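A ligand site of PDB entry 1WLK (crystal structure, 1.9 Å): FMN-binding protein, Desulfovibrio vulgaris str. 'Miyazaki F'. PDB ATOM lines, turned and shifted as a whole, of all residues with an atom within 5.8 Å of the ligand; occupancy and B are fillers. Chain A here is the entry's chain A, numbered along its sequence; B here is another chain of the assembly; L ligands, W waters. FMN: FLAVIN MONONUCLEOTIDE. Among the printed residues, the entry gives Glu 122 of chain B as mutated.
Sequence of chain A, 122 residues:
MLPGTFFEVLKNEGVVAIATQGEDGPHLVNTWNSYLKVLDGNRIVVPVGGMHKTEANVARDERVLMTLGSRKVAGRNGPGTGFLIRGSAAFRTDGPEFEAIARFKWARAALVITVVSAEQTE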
ATOM      1  N   VAL A  15     -11.925   0.120 -13.623  1.00  0.00           N
ATOM      2  CA  VAL A  15     -12.580   1.021 -12.696  1.00  0.00           C
ATOM      3  C   VAL A  15     -13.928   0.459 -12.261  1.00  0.00           C
ATOM      4  O   VAL A  15     -14.800   0.212 -13.088  1.00  0.00           O
ATOM      5  CB  VAL A  15     -12.789   2.398 -13.344  1.00  0.00           C
ATOM      6  CG1 VAL A  15     -13.525   3.331 -12.392  1.00  0.00           C
ATOM      7  CG2 VAL A  15     -11.435   2.986 -13.733  1.00  0.00           C
ATOM      8  N   HIS A  27     -25.619   8.953  -6.016  1.00  0.00           N
ATOM      9  CA  HIS A  27     -24.232   9.325  -5.813  1.00  0.00           C
ATOM     10  C   HIS A  27     -23.438   8.194  -6.431  1.00  0.00           C
ATOM     11  O   HIS A  27     -23.919   7.058  -6.487  1.00  0.00           O
ATOM     12  CB  HIS A  27     -23.855   9.497  -4.332  1.00  0.00           C
ATOM     13  CG  HIS A  27     -22.474  10.033  -4.150  1.00  0.00           C
ATOM     14  ND1 HIS A  27     -22.032  11.161  -4.805  1.00  0.00           N
ATOM     15  CD2 HIS A  27     -21.414   9.576  -3.437  1.00  0.00           C
ATOM     16  CE1 HIS A  27     -20.761  11.379  -4.499  1.00  0.00           C
ATOM     17  NE2 HIS A  27     -20.368  10.434  -3.677  1.00  0.00           N
ATOM     18  N   LEU A  28     -22.230   8.494  -6.890  1.00  0.00           N
ATOM     19  CA  LEU A  28     -21.411   7.486  -7.556  1.00  0.00           C
ATOM     20  C   LEU A  28     -19.944   7.624  -7.178  1.00  0.00           C
ATOM     21  O   LEU A  28     -19.383   8.720  -7.252  1.00  0.00           O
ATOM     22  CB  LEU A  28     -21.577   7.655  -9.072  1.00  0.00           C
ATOM     23  CG  LEU A  28     -21.037   6.601 -10.033  1.00  0.00           C
ATOM     24  CD1 LEU A  28     -21.693   5.279  -9.750  1.00  0.00           C
ATOM     25  CD2 LEU A  28     -21.305   7.032 -11.477  1.00  0.00           C
ATOM     26  N   VAL A  29     -19.324   6.524  -6.771  1.00  0.00           N
ATOM     27  CA  VAL A  29     -17.909   6.543  -6.415  1.00  0.00           C
ATOM     28  C   VAL A  29     -17.230   5.341  -7.027  1.00  0.00           C
ATOM     29  O   VAL A  29     -17.900   4.474  -7.601  1.00  0.00           O
ATOM     30  CB  VAL A  29     -17.693   6.555  -4.880  1.00  0.00           C
ATOM     31  CG1 VAL A  29     -18.289   7.832  -4.298  1.00  0.00           C
ATOM     32  CG2 VAL A  29     -18.295   5.327  -4.246  1.00  0.00           C
ATOM     33  N   ASN A  30     -15.906   5.254  -6.905  1.00  0.00           N
ATOM     34  CA  ASN A  30     -15.164   4.160  -7.515  1.00  0.00           C
ATOM     35  C   ASN A  30     -14.138   3.471  -6.633  1.00  0.00           C
ATOM     36  O   ASN A  30     -13.845   3.900  -5.518  1.00  0.00           O
ATOM     37  CB  ASN A  30     -14.397   4.663  -8.734  1.00  0.00           C
ATOM     38  CG  ASN A  30     -15.248   5.437  -9.709  1.00  0.00           C
ATOM     39  OD1 ASN A  30     -15.253   6.672  -9.725  1.00  0.00           O
ATOM     40  ND2 ASN A  30     -15.984   4.722 -10.546  1.00  0.00           N
ATOM     41  N   THR A  31     -13.606   2.375  -7.169  1.00  0.00           N
ATOM     42  CA  THR A  31     -12.520   1.617  -6.574  1.00  0.00           C
ATOM     43  C   THR A  31     -11.901   0.904  -7.776  1.00  0.00           C
ATOM     44  O   THR A  31     -12.393   1.076  -8.903  1.00  0.00           O
ATOM     45  CB  THR A  31     -12.955   0.596  -5.505  1.00  0.00           C
ATOM     46  OG1 THR A  31     -11.775  -0.001  -4.934  1.00  0.00           O
ATOM     47  CG2 THR A  31     -13.843  -0.487  -6.084  1.00  0.00           C
ATOM     48  N   TRP A  32     -10.829   0.151  -7.573  1.00  0.00           N
ATOM     49  CA  TRP A  32     -10.173  -0.546  -8.675  1.00  0.00           C
ATOM     50  C   TRP A  32     -10.478  -2.037  -8.685  1.00  0.00           C
ATOM     51  O   TRP A  32     -10.601  -2.660  -7.625  1.00  0.00           O
ATOM     52  CB  TRP A  32      -8.653  -0.367  -8.586  1.00  0.00           C
ATOM     53  CG  TRP A  32      -8.178   1.053  -8.653  1.00  0.00           C
ATOM     54  CD1 TRP A  32      -7.810   1.857  -7.603  1.00  0.00           C
ATOM     55  CD2 TRP A  32      -7.948   1.830  -9.835  1.00  0.00           C
ATOM     56  NE1 TRP A  32      -7.371   3.072  -8.067  1.00  0.00           N
ATOM     57  CE2 TRP A  32      -7.441   3.078  -9.435  1.00  0.00           C
ATOM     58  CE3 TRP A  32      -8.114   1.582 -11.211  1.00  0.00           C
ATOM     59  CZ2 TRP A  32      -7.094   4.089 -10.350  1.00  0.00           C
ATOM     60  CZ3 TRP A  32      -7.782   2.575 -12.121  1.00  0.00           C
ATOM     61  CH2 TRP A  32      -7.276   3.810 -11.682  1.00  0.00           C
ATOM     62  N   TYR A  35      -8.554  -4.125  -6.368  1.00  0.00           N
ATOM     63  CA  TYR A  35      -8.720  -3.918  -4.930  1.00  0.00           C
ATOM     64  C   TYR A  35      -9.806  -4.803  -4.329  1.00  0.00           C
ATOM     65  O   TYR A  35      -9.803  -5.080  -3.133  1.00  0.00           O
ATOM     66  CB  TYR A  35      -9.082  -2.462  -4.625  1.00  0.00           C
ATOM     67  CG  TYR A  35      -7.954  -1.473  -4.753  1.00  0.00           C
ATOM     68  CD1 TYR A  35      -8.111  -0.163  -4.297  1.00  0.00           C
ATOM     69  CD2 TYR A  35      -6.730  -1.828  -5.317  1.00  0.00           C
ATOM     70  CE1 TYR A  35      -7.084   0.774  -4.403  1.00  0.00           C
ATOM     71  CE2 TYR A  35      -5.700  -0.898  -5.438  1.00  0.00           C
ATOM     72  CZ  TYR A  35      -5.882   0.397  -4.972  1.00  0.00           C
ATOM     73  OH  TYR A  35      -4.865   1.325  -5.068  1.00  0.00           O
ATOM     74  N   VAL A  46     -14.619  -3.875  -0.285  1.00  0.00           N
ATOM     75  CA  VAL A  46     -13.931  -2.747  -0.898  1.00  0.00           C
ATOM     76  C   VAL A  46     -13.168  -1.920   0.146  1.00  0.00           C
ATOM     77  O   VAL A  46     -13.743  -1.527   1.160  1.00  0.00           O
ATOM     78  CB  VAL A  46     -14.937  -1.801  -1.604  1.00  0.00           C
ATOM     79  CG1 VAL A  46     -14.205  -0.588  -2.186  1.00  0.00           C
ATOM     80  CG2 VAL A  46     -15.693  -2.556  -2.694  1.00  0.00           C
ATOM     81  N   PRO A  47     -11.880  -1.642  -0.104  1.00  0.00           N
ATOM     82  CA  PRO A  47     -11.087  -0.845   0.849  1.00  0.00           C
ATOM     83  C   PRO A  47     -11.581   0.590   0.778  1.00  0.00           C
ATOM     84  O   PRO A  47     -11.604   1.196  -0.289  1.00  0.00           O
ATOM     85  CB  PRO A  47      -9.663  -1.011   0.327  1.00  0.00           C
ATOM     86  CG  PRO A  47      -9.861  -1.115  -1.142  1.00  0.00           C
ATOM     87  CD  PRO A  47     -11.061  -2.034  -1.270  1.00  0.00           C
ATOM     88  N   VAL A  48     -11.973   1.133   1.933  1.00  0.00           N
ATOM     89  CA  VAL A  48     -12.485   2.496   1.990  1.00  0.00           C
ATOM     90  C   VAL A  48     -11.490   3.516   2.524  1.00  0.00           C
ATOM     91  O   VAL A  48     -10.971   3.371   3.636  1.00  0.00           O
ATOM     92  CB  VAL A  48     -13.751   2.563   2.892  1.00  0.00           C
ATOM     93  CG1 VAL A  48     -14.158   4.010   3.124  1.00  0.00           C
ATOM     94  CG2 VAL A  48     -14.890   1.789   2.239  1.00  0.00           C
ATOM     95  N   GLY A  49     -11.213   4.525   1.716  1.00  0.00           N
ATOM     96  CA  GLY A  49     -10.325   5.602   2.110  1.00  0.00           C
ATOM     97  C   GLY A  49     -11.229   6.794   2.386  1.00  0.00           C
ATOM     98  O   GLY A  49     -11.229   7.341   3.493  1.00  0.00           O
ATOM     99  N   GLY A  50     -11.997   7.191   1.390  1.00  0.00           N
ATOM    100  CA  GLY A  50     -12.917   8.291   1.546  1.00  0.00           C
ATOM    101  C   GLY A  50     -14.322   7.747   1.719  1.00  0.00           C
ATOM    102  O   GLY A  50     -14.690   7.278   2.799  1.00  0.00           O
ATOM    103  N   MET A  51     -15.109   7.805   0.643  1.00  0.00           N
ATOM    104  CA  MET A  51     -16.484   7.332   0.638  1.00  0.00           C
ATOM    105  C   MET A  51     -17.282   7.791   1.852  1.00  0.00           C
ATOM    106  O   MET A  51     -17.925   6.992   2.534  1.00  0.00           O
ATOM    107  CB  MET A  51     -16.517   5.803   0.543  1.00  0.00           C
ATOM    108  CG  MET A  51     -15.922   5.288  -0.751  1.00  0.00           C
ATOM    109  SD  MET A  51     -16.236   3.541  -1.054  1.00  0.00           S
ATOM    110  CE  MET A  51     -15.104   3.241  -2.399  1.00  0.00           C
ATOM    111  N   HIS A  52     -17.248   9.093   2.088  1.00  0.00           N
ATOM    112  CA  HIS A  52     -17.953   9.686   3.219  1.00  0.00           C
ATOM    113  C   HIS A  52     -19.420   9.929   2.867  1.00  0.00           C
ATOM    114  O   HIS A  52     -20.313   9.567   3.639  1.00  0.00           O
ATOM    115  CB  HIS A  52     -17.259  10.980   3.618  1.00  0.00           C
ATOM    116  CG  HIS A  52     -15.824  10.783   3.990  1.00  0.00           C
ATOM    117  ND1 HIS A  52     -15.442  10.052   5.090  1.00  0.00           N
ATOM    118  CD2 HIS A  52     -14.679  11.161   3.368  1.00  0.00           C
ATOM    119  CE1 HIS A  52     -14.120   9.981   5.140  1.00  0.00           C
ATOM    120  NE2 HIS A  52     -13.635  10.656   4.107  1.00  0.00           N
ATOM    121  N   LYS A  53     -19.671  10.538   1.721  1.00  0.00           N
ATOM    122  CA  LYS A  53     -21.042  10.780   1.299  1.00  0.00           C
ATOM    123  C   LYS A  53     -21.671   9.403   1.071  1.00  0.00           C
ATOM    124  O   LYS A  53     -22.842   9.165   1.403  1.00  0.00           O
ATOM    125  CB  LYS A  53     -21.041  11.598  -0.001  1.00  0.00           C
ATOM    126  CG  LYS A  53     -22.159  11.264  -0.957  1.00  0.00           C
ATOM    127  CD  LYS A  53     -23.404  12.127  -0.825  1.00  0.00           C
ATOM    128  CE  LYS A  53     -24.429  11.699  -1.884  1.00  0.00           C
ATOM    129  NZ  LYS A  53     -25.625  12.567  -1.967  1.00  0.00           N
ATOM    130  N   THR A  54     -20.873   8.479   0.530  1.00  0.00           N
ATOM    131  CA  THR A  54     -21.338   7.127   0.263  1.00  0.00           C
ATOM    132  C   THR A  54     -21.749   6.435   1.565  1.00  0.00           C
ATOM    133  O   THR A  54     -22.829   5.830   1.640  1.00  0.00           O
ATOM    134  CB  THR A  54     -20.225   6.294  -0.425  1.00  0.00           C
ATOM    135  OG1 THR A  54     -19.944   6.859  -1.711  1.00  0.00           O
ATOM    136  CG2 THR A  54     -20.662   4.846  -0.598  1.00  0.00           C
ATOM    137  N   GLU A  55     -20.917   6.540   2.583  1.00  0.00           N
ATOM    138  CA  GLU A  55     -21.206   5.941   3.878  1.00  0.00           C
ATOM    139  C   GLU A  55     -22.485   6.512   4.480  1.00  0.00           C
ATOM    140  O   GLU A  55     -23.285   5.788   5.077  1.00  0.00           O
ATOM    141  CB  GLU A  55     -20.037   6.152   4.842  1.00  0.00           C
ATOM    142  CG  GLU A  55     -20.355   5.795   6.295  1.00  0.00           C
ATOM    143  CD  GLU A  55     -19.112   5.677   7.150  1.00  0.00           C
ATOM    144  OE1 GLU A  55     -18.121   6.384   6.885  1.00  0.00           O
ATOM    145  OE2 GLU A  55     -19.132   4.862   8.103  1.00  0.00           O
ATOM    146  N   TRP A 106      -4.094   2.597   4.143  1.00  0.00           N
ATOM    147  CA  TRP A 106      -4.874   3.831   4.056  1.00  0.00           C
ATOM    148  C   TRP A 106      -6.369   3.589   4.272  1.00  0.00           C
ATOM    149  O   TRP A 106      -7.155   4.540   4.357  1.00  0.00           O
ATOM    150  CB  TRP A 106      -4.663   4.502   2.702  1.00  0.00           C
ATOM    151  CG  TRP A 106      -4.774   3.562   1.534  1.00  0.00           C
ATOM    152  CD1 TRP A 106      -3.740   2.896   0.924  1.00  0.00           C
ATOM    153  CD2 TRP A 106      -5.972   3.157   0.859  1.00  0.00           C
ATOM    154  NE1 TRP A 106      -4.225   2.105  -0.091  1.00  0.00           N
ATOM    155  CE2 TRP A 106      -5.589   2.239  -0.158  1.00  0.00           C
ATOM    156  CE3 TRP A 106      -7.330   3.472   1.003  1.00  0.00           C
ATOM    157  CZ2 TRP A 106      -6.522   1.647  -1.023  1.00  0.00           C
ATOM    158  CZ3 TRP A 106      -8.253   2.873   0.143  1.00  0.00           C
ATOM    159  CH2 TRP A 106      -7.845   1.973  -0.859  1.00  0.00           C
ATOM    160  N   LEU B  68     -15.157   7.482 -14.760  1.00  0.00           N
ATOM    161  CA  LEU B  68     -14.295   6.785 -15.697  1.00  0.00           C
ATOM    162  C   LEU B  68     -12.858   7.031 -15.214  1.00  0.00           C
ATOM    163  O   LEU B  68     -12.599   7.986 -14.497  1.00  0.00           O
ATOM    164  CB  LEU B  68     -14.470   7.326 -17.121  1.00  0.00           C
ATOM    165  CG  LEU B  68     -13.987   8.759 -17.400  1.00  0.00           C
ATOM    166  CD1 LEU B  68     -14.014   9.037 -18.897  1.00  0.00           C
ATOM    167  CD2 LEU B  68     -14.850   9.771 -16.652  1.00  0.00           C
ATOM    168  N   GLY B  69     -11.944   6.161 -15.609  1.00  0.00           N
ATOM    169  CA  GLY B  69     -10.566   6.355 -15.194  1.00  0.00           C
ATOM    170  C   GLY B  69      -9.634   5.387 -15.869  1.00  0.00           C
ATOM    171  O   GLY B  69     -10.050   4.629 -16.748  1.00  0.00           O
ATOM    172  N   SER B  70      -8.370   5.390 -15.449  1.00  0.00           N
ATOM    173  CA  SER B  70      -7.383   4.489 -16.026  1.00  0.00           C
ATOM    174  C   SER B  70      -6.181   4.388 -15.095  1.00  0.00           C
ATOM    175  O   SER B  70      -5.688   5.398 -14.603  1.00  0.00           O
ATOM    176  CB  SER B  70      -6.930   4.994 -17.395  1.00  0.00           C
ATOM    177  OG  SER B  70      -5.915   4.159 -17.934  1.00  0.00           O
ATOM    178  N   THR B  81      -5.793   7.293 -12.135  1.00  0.00           N
ATOM    179  CA  THR B  81      -6.628   8.472 -11.927  1.00  0.00           C
ATOM    180  C   THR B  81      -8.025   8.250 -12.500  1.00  0.00           C
ATOM    181  O   THR B  81      -8.282   7.240 -13.165  1.00  0.00           O
ATOM    182  CB  THR B  81      -6.020   9.719 -12.589  1.00  0.00           C
ATOM    183  OG1 THR B  81      -6.681  10.899 -12.105  1.00  0.00           O
ATOM    184  CG2 THR B  81      -6.175   9.653 -14.095  1.00  0.00           C
ATOM    185  N   GLY B  82      -8.903   9.203 -12.255  1.00  0.00           N
ATOM    186  CA  GLY B  82     -10.261   9.100 -12.756  1.00  0.00           C
ATOM    187  C   GLY B  82     -11.055  10.345 -12.425  1.00  0.00           C
ATOM    188  O   GLY B  82     -10.564  11.221 -11.689  1.00  0.00           O
ATOM    189  N   PHE B  83     -12.273  10.420 -12.966  1.00  0.00           N
ATOM    190  CA  PHE B  83     -13.126  11.586 -12.761  1.00  0.00           C
ATOM    191  C   PHE B  83     -14.575  11.283 -12.438  1.00  0.00           C
ATOM    192  O   PHE B  83     -15.117  10.250 -12.862  1.00  0.00           O
ATOM    193  CB  PHE B  83     -13.153  12.462 -14.014  1.00  0.00           C
ATOM    194  CG  PHE B  83     -11.830  13.032 -14.404  1.00  0.00           C
ATOM    195  CD1 PHE B  83     -10.895  12.248 -15.070  1.00  0.00           C
ATOM    196  CD2 PHE B  83     -11.506  14.345 -14.087  1.00  0.00           C
ATOM    197  CE1 PHE B  83      -9.651  12.772 -15.418  1.00  0.00           C
ATOM    198  CE2 PHE B  83     -10.266  14.880 -14.428  1.00  0.00           C
ATOM    199  CZ  PHE B  83      -9.336  14.088 -15.097  1.00  0.00           C
ATOM    200  N   THR B 121     -11.173  12.750  -8.990  1.00  0.00           N
ATOM    201  CA  THR B 121     -11.332  12.151  -7.682  1.00  0.00           C
ATOM    202  C   THR B 121     -10.200  11.245  -7.204  1.00  0.00           C
ATOM    203  O   THR B 121     -10.297  10.653  -6.136  1.00  0.00           O
ATOM    204  CB  THR B 121     -12.630  11.346  -7.628  1.00  0.00           C
ATOM    205  OG1 THR B 121     -12.705  10.503  -8.791  1.00  0.00           O
ATOM    206  CG2 THR B 121     -13.813  12.289  -7.609  1.00  0.00           C
ATOM    207  N   GLU B 122      -9.142  11.138  -7.994  1.00  0.00           N
ATOM    208  CA  GLU B 122      -7.994  10.336  -7.595  1.00  0.00           C
ATOM    209  C   GLU B 122      -6.766  10.709  -8.421  1.00  0.00           C
ATOM    210  O   GLU B 122      -6.955  11.228  -9.534  1.00  0.00           O
ATOM    211  CB  GLU B 122      -8.292   8.846  -7.753  1.00  0.00           C
ATOM    212  CG  GLU B 122      -7.101   7.968  -7.402  1.00  0.00           C
ATOM    213  CD  GLU B 122      -7.478   6.733  -6.609  1.00  0.00           C
ATOM    214  OE1 GLU B 122      -8.282   6.853  -5.660  1.00  0.00           O
ATOM    215  OE2 GLU B 122      -6.942   5.654  -6.934  1.00  0.00           O
ATOM    216  OXT GLU B 122      -5.643  10.467  -7.938  1.00  0.00           O
HETATM  217  N1  FMN L   1     -12.012   5.853  -2.793  1.00  0.00           N
HETATM  218  C2  FMN L   1     -11.875   4.920  -1.799  1.00  0.00           C
HETATM  219  O2  FMN L   1     -12.230   5.145  -0.635  1.00  0.00           O
HETATM  220  N3  FMN L   1     -11.326   3.657  -2.124  1.00  0.00           N
HETATM  221  C4  FMN L   1     -10.903   3.273  -3.370  1.00  0.00           C
HETATM  222  O4  FMN L   1     -10.424   2.142  -3.568  1.00  0.00           O
HETATM  223  C4A FMN L   1     -11.046   4.270  -4.434  1.00  0.00           C
HETATM  224  N5  FMN L   1     -10.652   3.954  -5.696  1.00  0.00           N
HETATM  225  C5A FMN L   1     -10.835   4.884  -6.714  1.00  0.00           C
HETATM  226  C6  FMN L   1     -10.482   4.546  -8.057  1.00  0.00           C
HETATM  227  C7  FMN L   1     -10.662   5.446  -9.124  1.00  0.00           C
HETATM  228  C7M FMN L   1     -10.287   5.047 -10.525  1.00  0.00           C
HETATM  229  C8  FMN L   1     -11.203   6.759  -8.822  1.00  0.00           C
HETATM  230  C8M FMN L   1     -11.421   7.781  -9.947  1.00  0.00           C
HETATM  231  C9  FMN L   1     -11.552   7.099  -7.525  1.00  0.00           C
HETATM  232  C9A FMN L   1     -11.395   6.205  -6.438  1.00  0.00           C
HETATM  233  N10 FMN L   1     -11.764   6.487  -5.084  1.00  0.00           N
HETATM  234  C10 FMN L   1     -11.607   5.546  -4.065  1.00  0.00           C
HETATM  235  C1' FMN L   1     -12.355   7.802  -4.712  1.00  0.00           C
HETATM  236  C2' FMN L   1     -13.887   7.672  -4.626  1.00  0.00           C
HETATM  237  O2' FMN L   1     -14.420   7.417  -5.916  1.00  0.00           O
HETATM  238  C3' FMN L   1     -14.549   8.892  -3.987  1.00  0.00           C
HETATM  239  O3' FMN L   1     -14.265  10.030  -4.837  1.00  0.00           O
HETATM  240  C4' FMN L   1     -14.038   9.215  -2.590  1.00  0.00           C
HETATM  241  O4' FMN L   1     -13.828   8.041  -1.788  1.00  0.00           O
HETATM  242  C5' FMN L   1     -15.018  10.105  -1.827  1.00  0.00           C
HETATM  243  O5' FMN L   1     -16.243   9.384  -1.614  1.00  0.00           O
HETATM  244  P   FMN L   1     -17.614  10.183  -1.322  1.00  0.00           P
HETATM  245  O1P FMN L   1     -17.856  11.066  -2.520  1.00  0.00           O
HETATM  246  O2P FMN L   1     -17.403  11.002  -0.057  1.00  0.00           O
HETATM  247  O3P FMN L   1     -18.644   9.111  -1.134  1.00  0.00           O
HETATM  248  O   HOH W   1     -18.344  13.766  -2.606  1.00  0.00           O
HETATM  249  O   HOH W   2      -8.218   5.349  -3.263  1.00  0.00           O
HETATM  250  O   HOH W   3     -14.848   8.932  -8.183  1.00  0.00           O
HETATM  251  O   HOH W   4     -10.538   9.064  -1.782  1.00  0.00           O
HETATM  252  O   HOH W   5      -9.345   6.798  -0.885  1.00  0.00           O
HETATM  253  O   HOH W   6     -16.583  11.390  -4.883  1.00  0.00           O
HETATM  254  O   HOH W   7     -12.117  11.922  -4.107  1.00  0.00           O
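CG2 of Val 15 touches C7M of the ligand, 3.98 Å away.
CG1 of Val 29 touches O3P of the ligand, 3.4 Å away.
Trp 32 touches the ligand.
CD1 of Tyr 35 touches O4 of the ligand (3.3 Å).
Val 48 touches the ligand.
CH2 of Trp 106 touches O4 of the ligand (3.7 Å).
O of Thr 81 of chain B touches C7M of the ligand (3.97 Å).
CA of Gly 82 of chain B touches C8M of the ligand, at 3.3 Å.
OG1 of Thr 121 of chain B touches C8M of the ligand, 3.2 Å away.
OE1 of Glu 122 of chain B touches C9A of the ligand (3.3 Å).
The backbone NH (N) of Ser 70 of chain B sits at hydrogen-bond distance from the backbone carbonyl oxygen (O) of Thr 81 of chain B, 2.9 Å away.
The backbone NH (N) of Thr 121 of chain B is in hydrogen-bond range of the backbone carbonyl oxygen (O) of Gly 82 of chain B, at 3.2 Å.
O of Glu 122 of chain B sits at hydrogen-bond distance from OG1 of Thr 81 of chain B, 2.6 Å away.
The side-chain carboxylate of Glu 122 of chain B lies within hydrogen-bond range of the indole nitrogen of Trp 32, at 2.9 Å.
Water W3 lies within hydrogen-bond range of OG1 of Thr 121 of chain B (2.7 Å), O2' of the ligand (2.8 Å) and OD1 of Asn 30 (2.8 Å).
Water W7 bridges an oxygen (O3') of the ligand (3.0 Å) and the backbone carbonyl oxygen (O) of Thr 121 of chain B (3.0 Å).
The backbone NH of Gly 50 is in hydrogen-bond range of an oxygen (O2) of the ligand (2.9 Å).
The backbone NH of His 52 lies within hydrogen-bond range of an oxygen (O2P) of the ligand, 2.9 Å away.
The side-chain hydroxyl (OG1) of Thr 31 is in hydrogen-bond range of an oxygen (O4) of the ligand (2.9 Å).
The backbone NH (N) of Gly 49 sits at hydrogen-bond distance from an oxygen (O2) of the ligand, 2.6 Å away.
O of Pro 47 lies within hydrogen-bond range of N3 of the ligand (3.1 Å).
An oxygen (O3P) of the ligand is in hydrogen-bond range of the backbone NH of Thr 54, 2.9 Å away.
The backbone NH (N) of Met 51 is in hydrogen-bond range of an oxygen (O4') of the ligand.
An oxygen (O2') of the ligand sits at hydrogen-bond distance from the backbone NH of Asn 30 (2.8 Å).
A ring nitrogen (NE2) of His 27 lies within hydrogen-bond range of an oxygen (O1P) of the ligand (2.8 Å).
OG1 of Thr 54 is in hydrogen-bond range of O3P of the ligand, 2.7 Å away.
An oxygen (O2P) of the ligand is in hydrogen-bond range of the backbone NH of Lys 53, 2.9 Å away.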
